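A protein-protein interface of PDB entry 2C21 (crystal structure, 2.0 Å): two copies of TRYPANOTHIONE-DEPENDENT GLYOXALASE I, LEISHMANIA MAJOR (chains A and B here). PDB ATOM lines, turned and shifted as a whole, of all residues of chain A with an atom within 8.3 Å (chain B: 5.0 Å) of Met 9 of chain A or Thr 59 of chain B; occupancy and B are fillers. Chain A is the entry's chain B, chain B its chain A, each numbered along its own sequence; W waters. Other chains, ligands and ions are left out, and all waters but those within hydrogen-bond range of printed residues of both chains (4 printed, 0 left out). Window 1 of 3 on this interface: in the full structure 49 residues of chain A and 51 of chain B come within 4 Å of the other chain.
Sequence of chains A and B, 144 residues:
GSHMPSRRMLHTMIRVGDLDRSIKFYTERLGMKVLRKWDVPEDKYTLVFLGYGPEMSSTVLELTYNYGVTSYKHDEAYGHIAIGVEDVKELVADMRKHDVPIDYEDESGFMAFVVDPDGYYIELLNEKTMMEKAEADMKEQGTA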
ATOM      1  N   SER A   6       1.050  12.370 -31.484  1.00  0.00           N
ATOM      2  CA  SER A   6      -0.390  11.926 -31.525  1.00  0.00           C
ATOM      3  C   SER A   6      -0.562  10.400 -31.562  1.00  0.00           C
ATOM      4  O   SER A   6      -0.074   9.721 -32.482  1.00  0.00           O
ATOM      5  CB  SER A   6      -1.117  12.564 -32.719  1.00  0.00           C
ATOM      6  OG  SER A   6      -2.254  11.799 -33.095  1.00  0.00           O
ATOM      7  N   ARG A   7      -1.264   9.872 -30.552  1.00  0.00           N
ATOM      8  CA  ARG A   7      -1.432   8.432 -30.385  1.00  0.00           C
ATOM      9  C   ARG A   7      -2.869   8.091 -29.963  1.00  0.00           C
ATOM     10  O   ARG A   7      -3.562   8.901 -29.351  1.00  0.00           O
ATOM     11  CB  ARG A   7      -0.404   7.890 -29.383  1.00  0.00           C
ATOM     12  CG  ARG A   7       1.024   8.081 -29.853  1.00  0.00           C
ATOM     13  CD  ARG A   7       2.097   7.464 -28.961  1.00  0.00           C
ATOM     14  NE  ARG A   7       3.411   7.913 -29.428  1.00  0.00           N
ATOM     15  CZ  ARG A   7       4.557   7.821 -28.753  1.00  0.00           C
ATOM     16  NH1 ARG A   7       4.608   7.271 -27.547  1.00  0.00           N
ATOM     17  NH2 ARG A   7       5.671   8.280 -29.302  1.00  0.00           N
ATOM     18  N   ARG A   8      -3.321   6.891 -30.310  1.00  0.00           N
ATOM     19  CA  ARG A   8      -4.698   6.498 -30.018  1.00  0.00           C
ATOM     20  C   ARG A   8      -4.843   5.012 -29.798  1.00  0.00           C
ATOM     21  O   ARG A   8      -4.249   4.190 -30.506  1.00  0.00           O
ATOM     22  CB  ARG A   8      -5.614   6.953 -31.158  1.00  0.00           C
ATOM     23  CG  ARG A   8      -7.096   6.683 -30.947  1.00  0.00           C
ATOM     24  CD  ARG A   8      -7.946   7.407 -32.005  1.00  0.00           C
ATOM     25  NE  ARG A   8      -7.700   6.902 -33.363  1.00  0.00           N
ATOM     26  CZ  ARG A   8      -8.453   6.004 -34.008  1.00  0.00           C
ATOM     27  NH1 ARG A   8      -9.550   5.507 -33.457  1.00  0.00           N
ATOM     28  NH2 ARG A   8      -8.127   5.626 -35.236  1.00  0.00           N
ATOM     29  N   MET A   9      -5.661   4.663 -28.809  1.00  0.00           N
ATOM     30  CA  MET A   9      -6.026   3.290 -28.605  1.00  0.00           C
ATOM     31  C   MET A   9      -6.906   2.813 -29.779  1.00  0.00           C
ATOM     32  O   MET A   9      -7.987   3.350 -29.996  1.00  0.00           O
ATOM     33  CB  MET A   9      -6.741   3.122 -27.265  1.00  0.00           C
ATOM     34  CG  MET A   9      -6.866   1.678 -26.846  1.00  0.00           C
ATOM     35  SD  MET A   9      -7.459   1.512 -25.157  1.00  0.00           S
ATOM     36  CE  MET A   9      -6.037   2.087 -24.242  1.00  0.00           C
ATOM     37  N   LEU A  10      -6.445   1.818 -30.531  1.00  0.00           N
ATOM     38  CA  LEU A  10      -7.149   1.367 -31.749  1.00  0.00           C
ATOM     39  C   LEU A  10      -8.080   0.174 -31.537  1.00  0.00           C
ATOM     40  O   LEU A  10      -9.222   0.140 -32.025  1.00  0.00           O
ATOM     41  CB  LEU A  10      -6.130   1.011 -32.834  1.00  0.00           C
ATOM     42  CG  LEU A  10      -5.284   2.154 -33.374  1.00  0.00           C
ATOM     43  CD1 LEU A  10      -4.401   1.648 -34.543  1.00  0.00           C
ATOM     44  CD2 LEU A  10      -6.168   3.310 -33.804  1.00  0.00           C
ATOM     45  N   HIS A  11      -7.584  -0.822 -30.822  1.00  0.00           N
ATOM     46  CA  HIS A  11      -8.385  -1.988 -30.557  1.00  0.00           C
ATOM     47  C   HIS A  11      -7.801  -2.876 -29.476  1.00  0.00           C
ATOM     48  O   HIS A  11      -6.642  -2.714 -29.059  1.00  0.00           O
ATOM     49  CB  HIS A  11      -8.646  -2.792 -31.846  1.00  0.00           C
ATOM     50  CG  HIS A  11      -7.417  -3.356 -32.497  1.00  0.00           C
ATOM     51  ND1 HIS A  11      -6.857  -2.805 -33.630  1.00  0.00           N
ATOM     52  CD2 HIS A  11      -6.674  -4.452 -32.203  1.00  0.00           C
ATOM     53  CE1 HIS A  11      -5.818  -3.531 -34.002  1.00  0.00           C
ATOM     54  NE2 HIS A  11      -5.692  -4.542 -33.158  1.00  0.00           N
ATOM     55  N   THR A  12      -8.640  -3.809 -29.037  1.00  0.00           N
ATOM     56  CA  THR A  12      -8.244  -4.892 -28.160  1.00  0.00           C
ATOM     57  C   THR A  12      -8.493  -6.211 -28.890  1.00  0.00           C
ATOM     58  O   THR A  12      -9.536  -6.387 -29.505  1.00  0.00           O
ATOM     59  CB  THR A  12      -9.045  -4.822 -26.835  1.00  0.00           C
ATOM     60  OG1 THR A  12      -8.747  -3.580 -26.160  1.00  0.00           O
ATOM     61  CG2 THR A  12      -8.710  -5.991 -25.944  1.00  0.00           C
ATOM     62  N   GLU A  55     -13.072   1.929 -37.376  1.00  0.00           N
ATOM     63  CA  GLU A  55     -11.777   2.045 -36.712  1.00  0.00           C
ATOM     64  C   GLU A  55     -11.208   3.448 -36.798  1.00  0.00           C
ATOM     65  O   GLU A  55     -10.404   3.829 -35.962  1.00  0.00           O
ATOM     66  CB  GLU A  55     -10.768   1.066 -37.305  1.00  0.00           C
ATOM     67  CG  GLU A  55     -11.075  -0.380 -37.028  1.00  0.00           C
ATOM     68  CD  GLU A  55     -10.373  -1.314 -37.996  1.00  0.00           C
ATOM     69  OE1 GLU A  55      -9.207  -1.685 -37.725  1.00  0.00           O
ATOM     70  OE2 GLU A  55     -10.998  -1.682 -39.018  1.00  0.00           O
ATOM     71  N   SER A  57     -12.621   6.240 -36.241  1.00  0.00           N
ATOM     72  CA  SER A  57     -13.121   7.142 -35.197  1.00  0.00           C
ATOM     73  C   SER A  57     -13.487   6.451 -33.888  1.00  0.00           C
ATOM     74  O   SER A  57     -13.902   7.128 -32.951  1.00  0.00           O
ATOM     75  CB  SER A  57     -14.323   7.931 -35.724  1.00  0.00           C
ATOM     76  OG  SER A  57     -15.413   7.061 -35.931  1.00  0.00           O
ATOM     77  N   SER A  58     -13.318   5.123 -33.822  1.00  0.00           N
ATOM     78  CA  SER A  58     -13.632   4.331 -32.642  1.00  0.00           C
ATOM     79  C   SER A  58     -12.481   3.416 -32.271  1.00  0.00           C
ATOM     80  O   SER A  58     -11.637   3.090 -33.110  1.00  0.00           O
ATOM     81  CB  SER A  58     -14.851   3.425 -32.887  1.00  0.00           C
ATOM     82  OG  SER A  58     -16.040   4.192 -32.976  1.00  0.00           O
ATOM     83  N   THR A  59     -12.459   3.034 -30.998  1.00  0.00           N
ATOM     84  CA  THR A  59     -11.653   1.939 -30.519  1.00  0.00           C
ATOM     85  C   THR A  59     -12.543   0.690 -30.604  1.00  0.00           C
ATOM     86  O   THR A  59     -13.712   0.716 -30.206  1.00  0.00           O
ATOM     87  CB  THR A  59     -11.152   2.200 -29.087  1.00  0.00           C
ATOM     88  OG1 THR A  59     -10.428   3.441 -29.056  1.00  0.00           O
ATOM     89  CG2 THR A  59     -10.238   1.105 -28.635  1.00  0.00           C
ATOM     90  N   VAL A  60     -11.998  -0.399 -31.138  1.00  0.00           N
ATOM     91  CA  VAL A  60     -12.829  -1.538 -31.536  1.00  0.00           C
ATOM     92  C   VAL A  60     -12.337  -2.877 -30.972  1.00  0.00           C
ATOM     93  O   VAL A  60     -11.366  -2.936 -30.229  1.00  0.00           O
ATOM     94  CB  VAL A  60     -12.968  -1.595 -33.093  1.00  0.00           C
ATOM     95  CG1 VAL A  60     -13.390  -0.236 -33.630  1.00  0.00           C
ATOM     96  CG2 VAL A  60     -11.691  -2.066 -33.760  1.00  0.00           C
ATOM     97  N   ILE A  81     -13.102  -6.336 -21.077  1.00  0.00           N
ATOM     98  CA  ILE A  81     -13.467  -5.083 -21.713  1.00  0.00           C
ATOM     99  C   ILE A  81     -14.747  -4.578 -21.061  1.00  0.00           C
ATOM    100  O   ILE A  81     -15.614  -5.375 -20.666  1.00  0.00           O
ATOM    101  CB  ILE A  81     -13.624  -5.207 -23.249  1.00  0.00           C
ATOM    102  CG1 ILE A  81     -14.829  -6.066 -23.626  1.00  0.00           C
ATOM    103  CG2 ILE A  81     -12.347  -5.761 -23.865  1.00  0.00           C
ATOM    104  CD1 ILE A  81     -15.134  -6.062 -25.127  1.00  0.00           C
ATOM    105  N   ALA A  82     -14.858  -3.254 -20.964  1.00  0.00           N
ATOM    106  CA  ALA A  82     -16.049  -2.608 -20.435  1.00  0.00           C
ATOM    107  C   ALA A  82     -16.767  -1.793 -21.504  1.00  0.00           C
ATOM    108  O   ALA A  82     -16.138  -1.045 -22.249  1.00  0.00           O
ATOM    109  CB  ALA A  82     -15.695  -1.737 -19.271  1.00  0.00           C
ATOM    110  N   ARG B   8     -20.636   2.404 -26.293  1.00  0.00           N
ATOM    111  CA  ARG B   8     -19.249   2.743 -26.537  1.00  0.00           C
ATOM    112  C   ARG B   8     -18.330   1.842 -25.723  1.00  0.00           C
ATOM    113  O   ARG B   8     -18.624   1.522 -24.577  1.00  0.00           O
ATOM    114  CB  ARG B   8     -19.000   4.223 -26.198  1.00  0.00           C
ATOM    115  CG  ARG B   8     -17.615   4.737 -26.568  1.00  0.00           C
ATOM    116  CD  ARG B   8     -17.536   6.267 -26.434  1.00  0.00           C
ATOM    117  NE  ARG B   8     -17.827   6.729 -25.068  1.00  0.00           N
ATOM    118  CZ  ARG B   8     -16.923   7.090 -24.150  1.00  0.00           C
ATOM    119  NH1 ARG B   8     -15.622   7.089 -24.411  1.00  0.00           N
ATOM    120  NH2 ARG B   8     -17.330   7.489 -22.941  1.00  0.00           N
ATOM    121  N   MET B   9     -17.237   1.416 -26.347  1.00  0.00           N
ATOM    122  CA  MET B   9     -16.134   0.730 -25.659  1.00  0.00           C
ATOM    123  C   MET B   9     -15.471   1.713 -24.711  1.00  0.00           C
ATOM    124  O   MET B   9     -14.989   2.774 -25.153  1.00  0.00           O
ATOM    125  CB  MET B   9     -15.156   0.168 -26.694  1.00  0.00           C
ATOM    126  CG  MET B   9     -14.010  -0.584 -26.119  1.00  0.00           C
ATOM    127  SD  MET B   9     -13.064  -1.500 -27.350  1.00  0.00           S
ATOM    128  CE  MET B   9     -14.233  -2.803 -27.691  1.00  0.00           C
ATOM    129  N   LEU B  10     -15.440   1.389 -23.418  1.00  0.00           N
ATOM    130  CA  LEU B  10     -14.907   2.341 -22.435  1.00  0.00           C
ATOM    131  C   LEU B  10     -13.469   2.076 -22.043  1.00  0.00           C
ATOM    132  O   LEU B  10     -12.651   3.000 -21.974  1.00  0.00           O
ATOM    133  CB  LEU B  10     -15.777   2.364 -21.185  1.00  0.00           C
ATOM    134  CG  LEU B  10     -17.224   2.777 -21.417  1.00  0.00           C
ATOM    135  CD1 LEU B  10     -17.895   2.944 -20.072  1.00  0.00           C
ATOM    136  CD2 LEU B  10     -17.377   4.063 -22.253  1.00  0.00           C
ATOM    137  N   HIS B  11     -13.155   0.815 -21.766  1.00  0.00           N
ATOM    138  CA  HIS B  11     -11.789   0.452 -21.392  1.00  0.00           C
ATOM    139  C   HIS B  11     -11.526  -1.036 -21.460  1.00  0.00           C
ATOM    140  O   HIS B  11     -12.435  -1.822 -21.612  1.00  0.00           O
ATOM    141  CB  HIS B  11     -11.420   0.996 -19.989  1.00  0.00           C
ATOM    142  CG  HIS B  11     -12.265   0.466 -18.867  1.00  0.00           C
ATOM    143  ND1 HIS B  11     -13.273   1.202 -18.275  1.00  0.00           N
ATOM    144  CD2 HIS B  11     -12.226  -0.717 -18.208  1.00  0.00           C
ATOM    145  CE1 HIS B  11     -13.821   0.485 -17.311  1.00  0.00           C
ATOM    146  NE2 HIS B  11     -13.211  -0.685 -17.258  1.00  0.00           N
ATOM    147  N   MET B  32       0.927   7.841 -22.481  1.00  0.00           N
ATOM    148  CA  MET B  32      -0.382   7.960 -21.846  1.00  0.00           C
ATOM    149  C   MET B  32      -0.256   8.854 -20.621  1.00  0.00           C
ATOM    150  O   MET B  32       0.850   9.162 -20.182  1.00  0.00           O
ATOM    151  CB  MET B  32      -0.915   6.602 -21.392  1.00  0.00           C
ATOM    152  CG  MET B  32      -1.055   5.593 -22.480  1.00  0.00           C
ATOM    153  SD  MET B  32      -1.854   4.103 -21.880  1.00  0.00           S
ATOM    154  CE  MET B  32      -1.780   3.103 -23.375  1.00  0.00           C
ATOM    155  N   TYR B  52      -4.877   8.194 -23.527  1.00  0.00           N
ATOM    156  CA  TYR B  52      -4.437   9.312 -24.325  1.00  0.00           C
ATOM    157  C   TYR B  52      -5.448  10.448 -24.247  1.00  0.00           C
ATOM    158  O   TYR B  52      -5.266  11.500 -24.841  1.00  0.00           O
ATOM    159  CB  TYR B  52      -4.220   8.841 -25.766  1.00  0.00           C
ATOM    160  CG  TYR B  52      -3.048   7.889 -25.898  1.00  0.00           C
ATOM    161  CD1 TYR B  52      -1.756   8.334 -25.691  1.00  0.00           C
ATOM    162  CD2 TYR B  52      -3.236   6.546 -26.206  1.00  0.00           C
ATOM    163  CE1 TYR B  52      -0.672   7.481 -25.808  1.00  0.00           C
ATOM    164  CE2 TYR B  52      -2.155   5.678 -26.316  1.00  0.00           C
ATOM    165  CZ  TYR B  52      -0.879   6.146 -26.125  1.00  0.00           C
ATOM    166  OH  TYR B  52       0.208   5.301 -26.250  1.00  0.00           O
ATOM    167  N   SER B  57     -14.098  11.007 -23.519  1.00  0.00           N
ATOM    168  CA  SER B  57     -13.889  11.090 -24.969  1.00  0.00           C
ATOM    169  C   SER B  57     -12.969  10.009 -25.557  1.00  0.00           C
ATOM    170  O   SER B  57     -12.672  10.039 -26.747  1.00  0.00           O
ATOM    171  CB  SER B  57     -13.317  12.465 -25.293  1.00  0.00           C
ATOM    172  OG  SER B  57     -12.080  12.651 -24.622  1.00  0.00           O
ATOM    173  N   SER B  58     -12.517   9.070 -24.729  1.00  0.00           N
ATOM    174  CA  SER B  58     -11.495   8.093 -25.107  1.00  0.00           C
ATOM    175  C   SER B  58     -11.797   6.746 -24.510  1.00  0.00           C
ATOM    176  O   SER B  58     -12.477   6.655 -23.485  1.00  0.00           O
ATOM    177  CB  SER B  58     -10.118   8.461 -24.567  1.00  0.00           C
ATOM    178  OG  SER B  58      -9.722   9.740 -24.960  1.00  0.00           O
ATOM    179  N   THR B  59     -11.238   5.721 -25.145  1.00  0.00           N
ATOM    180  CA  THR B  59     -11.221   4.353 -24.622  1.00  0.00           C
ATOM    181  C   THR B  59      -9.850   4.161 -23.974  1.00  0.00           C
ATOM    182  O   THR B  59      -8.804   4.448 -24.579  1.00  0.00           O
ATOM    183  CB  THR B  59     -11.472   3.350 -25.762  1.00  0.00           C
ATOM    184  OG1 THR B  59     -12.736   3.653 -26.367  1.00  0.00           O
ATOM    185  CG2 THR B  59     -11.490   1.909 -25.257  1.00  0.00           C
ATOM    186  N   VAL B  60      -9.853   3.749 -22.717  1.00  0.00           N
ATOM    187  CA  VAL B  60      -8.658   3.824 -21.902  1.00  0.00           C
ATOM    188  C   VAL B  60      -8.209   2.447 -21.423  1.00  0.00           C
ATOM    189  O   VAL B  60      -8.799   1.425 -21.781  1.00  0.00           O
ATOM    190  CB  VAL B  60      -8.854   4.835 -20.735  1.00  0.00           C
ATOM    191  CG1 VAL B  60      -9.245   6.201 -21.293  1.00  0.00           C
ATOM    192  CG2 VAL B  60      -9.899   4.351 -19.710  1.00  0.00           C
ATOM    193  N   LEU B  61      -7.138   2.448 -20.636  1.00  0.00           N
ATOM    194  CA  LEU B  61      -6.565   1.264 -20.028  1.00  0.00           C
ATOM    195  C   LEU B  61      -6.777   1.322 -18.515  1.00  0.00           C
ATOM    196  O   LEU B  61      -6.534   2.362 -17.885  1.00  0.00           O
ATOM    197  CB  LEU B  61      -5.062   1.211 -20.348  1.00  0.00           C
ATOM    198  CG  LEU B  61      -4.234   0.042 -19.819  1.00  0.00           C
ATOM    199  CD1 LEU B  61      -4.801  -1.291 -20.294  1.00  0.00           C
ATOM    200  CD2 LEU B  61      -2.782   0.209 -20.270  1.00  0.00           C
ATOM    201  N   ILE B  81      -3.536  -5.139 -26.772  1.00  0.00           N
ATOM    202  CA  ILE B  81      -4.076  -3.858 -27.195  1.00  0.00           C
ATOM    203  C   ILE B  81      -3.165  -3.289 -28.304  1.00  0.00           C
ATOM    204  O   ILE B  81      -1.953  -3.532 -28.320  1.00  0.00           O
ATOM    205  CB  ILE B  81      -4.208  -2.810 -26.052  1.00  0.00           C
ATOM    206  CG1 ILE B  81      -2.849  -2.477 -25.433  1.00  0.00           C
ATOM    207  CG2 ILE B  81      -5.247  -3.268 -24.991  1.00  0.00           C
ATOM    208  CD1 ILE B  81      -2.859  -1.217 -24.567  1.00  0.00           C
ATOM    209  N   ALA B  82      -3.778  -2.555 -29.224  1.00  0.00           N
ATOM    210  CA  ALA B  82      -3.072  -1.940 -30.335  1.00  0.00           C
ATOM    211  C   ALA B  82      -3.169  -0.447 -30.185  1.00  0.00           C
ATOM    212  O   ALA B  82      -4.234   0.083 -29.856  1.00  0.00           O
ATOM    213  CB  ALA B  82      -3.691  -2.373 -31.645  1.00  0.00           C
ATOM    214  N   ILE B  83      -2.051   0.224 -30.444  1.00  0.00           N
ATOM    215  CA  ILE B  83      -1.955   1.661 -30.326  1.00  0.00           C
ATOM    216  C   ILE B  83      -1.463   2.209 -31.664  1.00  0.00           C
ATOM    217  O   ILE B  83      -0.472   1.728 -32.185  1.00  0.00           O
ATOM    218  CB  ILE B  83      -0.989   2.046 -29.180  1.00  0.00           C
ATOM    219  CG1 ILE B  83      -1.551   1.529 -27.831  1.00  0.00           C
ATOM    220  CG2 ILE B  83      -0.723   3.568 -29.166  1.00  0.00           C
ATOM    221  CD1 ILE B  83      -0.612   1.725 -26.652  1.00  0.00           C
HETATM  222  O   HOH W   1      -9.263  -0.162 -24.469  1.00  0.00           O
HETATM  223  O   HOH W   2     -10.744  -2.228 -27.239  1.00  0.00           O
HETATM  224  O   HOH W   3      -9.926   5.982 -27.837  1.00  0.00           O
HETATM  225  O   HOH W   4     -14.538   4.076 -29.112  1.00  0.00           O
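N of Ala 82 of chain A sits at hydrogen-bond distance from O of His 11 of chain B (2.9 Å).
SD of Met 9 of chain B sits close to O of Val 60 of chain A, 3.6 Å away.
SD of Met 9 of chain B lies close to O of Thr 59 of chain A.
N of Ala 82 of chain B lies within hydrogen-bond range of O of His 11 of chain A, at 2.9 Å.
The side-chain sulfur of Met 9 of chain A lies close to the backbone carbonyl oxygen of Thr 59 of chain B.
The backbone NH (N) of Leu 10 of chain A lies within hydrogen-bond range of the backbone carbonyl oxygen (O) of Ala 82 of chain B, 2.9 Å away.
The side-chain sulfur (SD) of Met 9 of chain A sits close to the backbone carbonyl oxygen (O) of Val 60 of chain B, 3.6 Å away.
N of Leu 10 of chain B is in hydrogen-bond range of O of Ala 82 of chain A (2.8 Å).
NH1 of Arg 8 of chain A is in hydrogen-bond range of O of Ser 58 of chain A (3.2 Å).
O of Glu 55 of chain A is in hydrogen-bond range of NH2 of Arg 8 of chain A (3.0 Å).
O of Leu 10 of chain B sits at hydrogen-bond distance from N of Val 60 of chain B (3.0 Å).
OG1 of Thr 59 of chain B is in hydrogen-bond range of O of Met 9 of chain B, 2.7 Å away.
O of Met 9 of chain A is in hydrogen-bond range of OG1 of Thr 59 of chain A, 2.6 Å away.
N of Val 60 of chain A is in hydrogen-bond range of O of Leu 10 of chain A, 3.0 Å away.
Among the printed residues, pairs that only touch across the chains: His 11 of chain A with Ile 81 of chain B, Arg 8 of chain A with Ile 83 of chain B, Ile 81 of chain A with His 11 of chain B, Thr 59 of chain A with Thr 59 of chain B, Arg 7 of chain A with Tyr 52 of chain B, Thr 12 of chain A with Ile 81 of chain B, Ala 82 of chain A with Met 9 of chain B, Met 9 of chain A with Leu 61 of chain B and Met 9 of chain A with Ala 82 of chain B.
Printed residues of chain B within 4 Å of Met 9 of chain A: Thr 59 (3.3 Å), Val 60 (3.6 Å), Leu 61 (3.8 Å) and Ala 82 (3.8 Å).
Of the printed residues of chain B, Val 60 of chain A touches Met 9 (3.6 Å).
Of the printed residues of chain B, Thr 59 of chain A touches Met 9 and Thr 59.
Of the printed residues of chain A, His 11 of chain B touches Ile 81 and Ala 82.
Of the printed residues of chain A, Ile 81 of chain B touches His 11 (3.4 Å) and Thr 12 (3.7 Å).
Printed residues of chain B within 4 Å of Leu 10 of chain A: Ala 82 (2.9 Å).
The nearest printed residue of chain B that does not touch Met 9 of chain A is Tyr 52 of chain B (4.03 Å).
The nearest printed residue of chain A that does not touch Thr 59 of chain B is Ser 58 of chain A (5.9 Å).
Hydrophobic or aromatic side chains of chain B within 4 Å of the printed part of chain A: Met 9, Leu 10, His 11, Tyr 52, Ile 81, Ala 82 and Ile 83.
Met 9 of chain A touches Val 60 of chain B, and with the chains exchanged Val 60 of chain A touches Met 9 of chain B.
Met 9 of chain A touches Ala 82 of chain B, and with the chains exchanged Ala 82 of chain A touches Met 9 of chain B.
His 11 of chain A touches Ile 81 of chain B, and with the chains exchanged Ile 81 of chain A touches His 11 of chain B.
His 11 of chain A touches Ala 82 of chain B, and with the chains exchanged Ala 82 of chain A touches His 11 of chain B.
Of the 17 pairs that touch across the chains among the printed residues, 13 have their exchanged pair printed and touching as well.
Water W2 lies within hydrogen-bond range of the side-chain sulfur (SD) of Met 9 of chain B (2.4 Å), the side-chain hydroxyl (OG1) of Thr 12 of chain A (2.6 Å) and the backbone carbonyl oxygen (O) of Val 60 of chain A (3.1 Å).
Water W1 lies within hydrogen-bond range of the side-chain sulfur of Met 9 of chain A (2.6 Å) and the backbone carbonyl oxygen of Val 60 of chain B (3.2 Å).
Water W3 lies within hydrogen-bond range of OG1 of Thr 59 of chain A and N of Thr 59 of chain B.
Water W4 bridges the backbone NH (N) of Thr 59 of chain A (3.0 Å) and the side-chain hydroxyl (OG1) of Thr 59 of chain B (3.3 Å).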
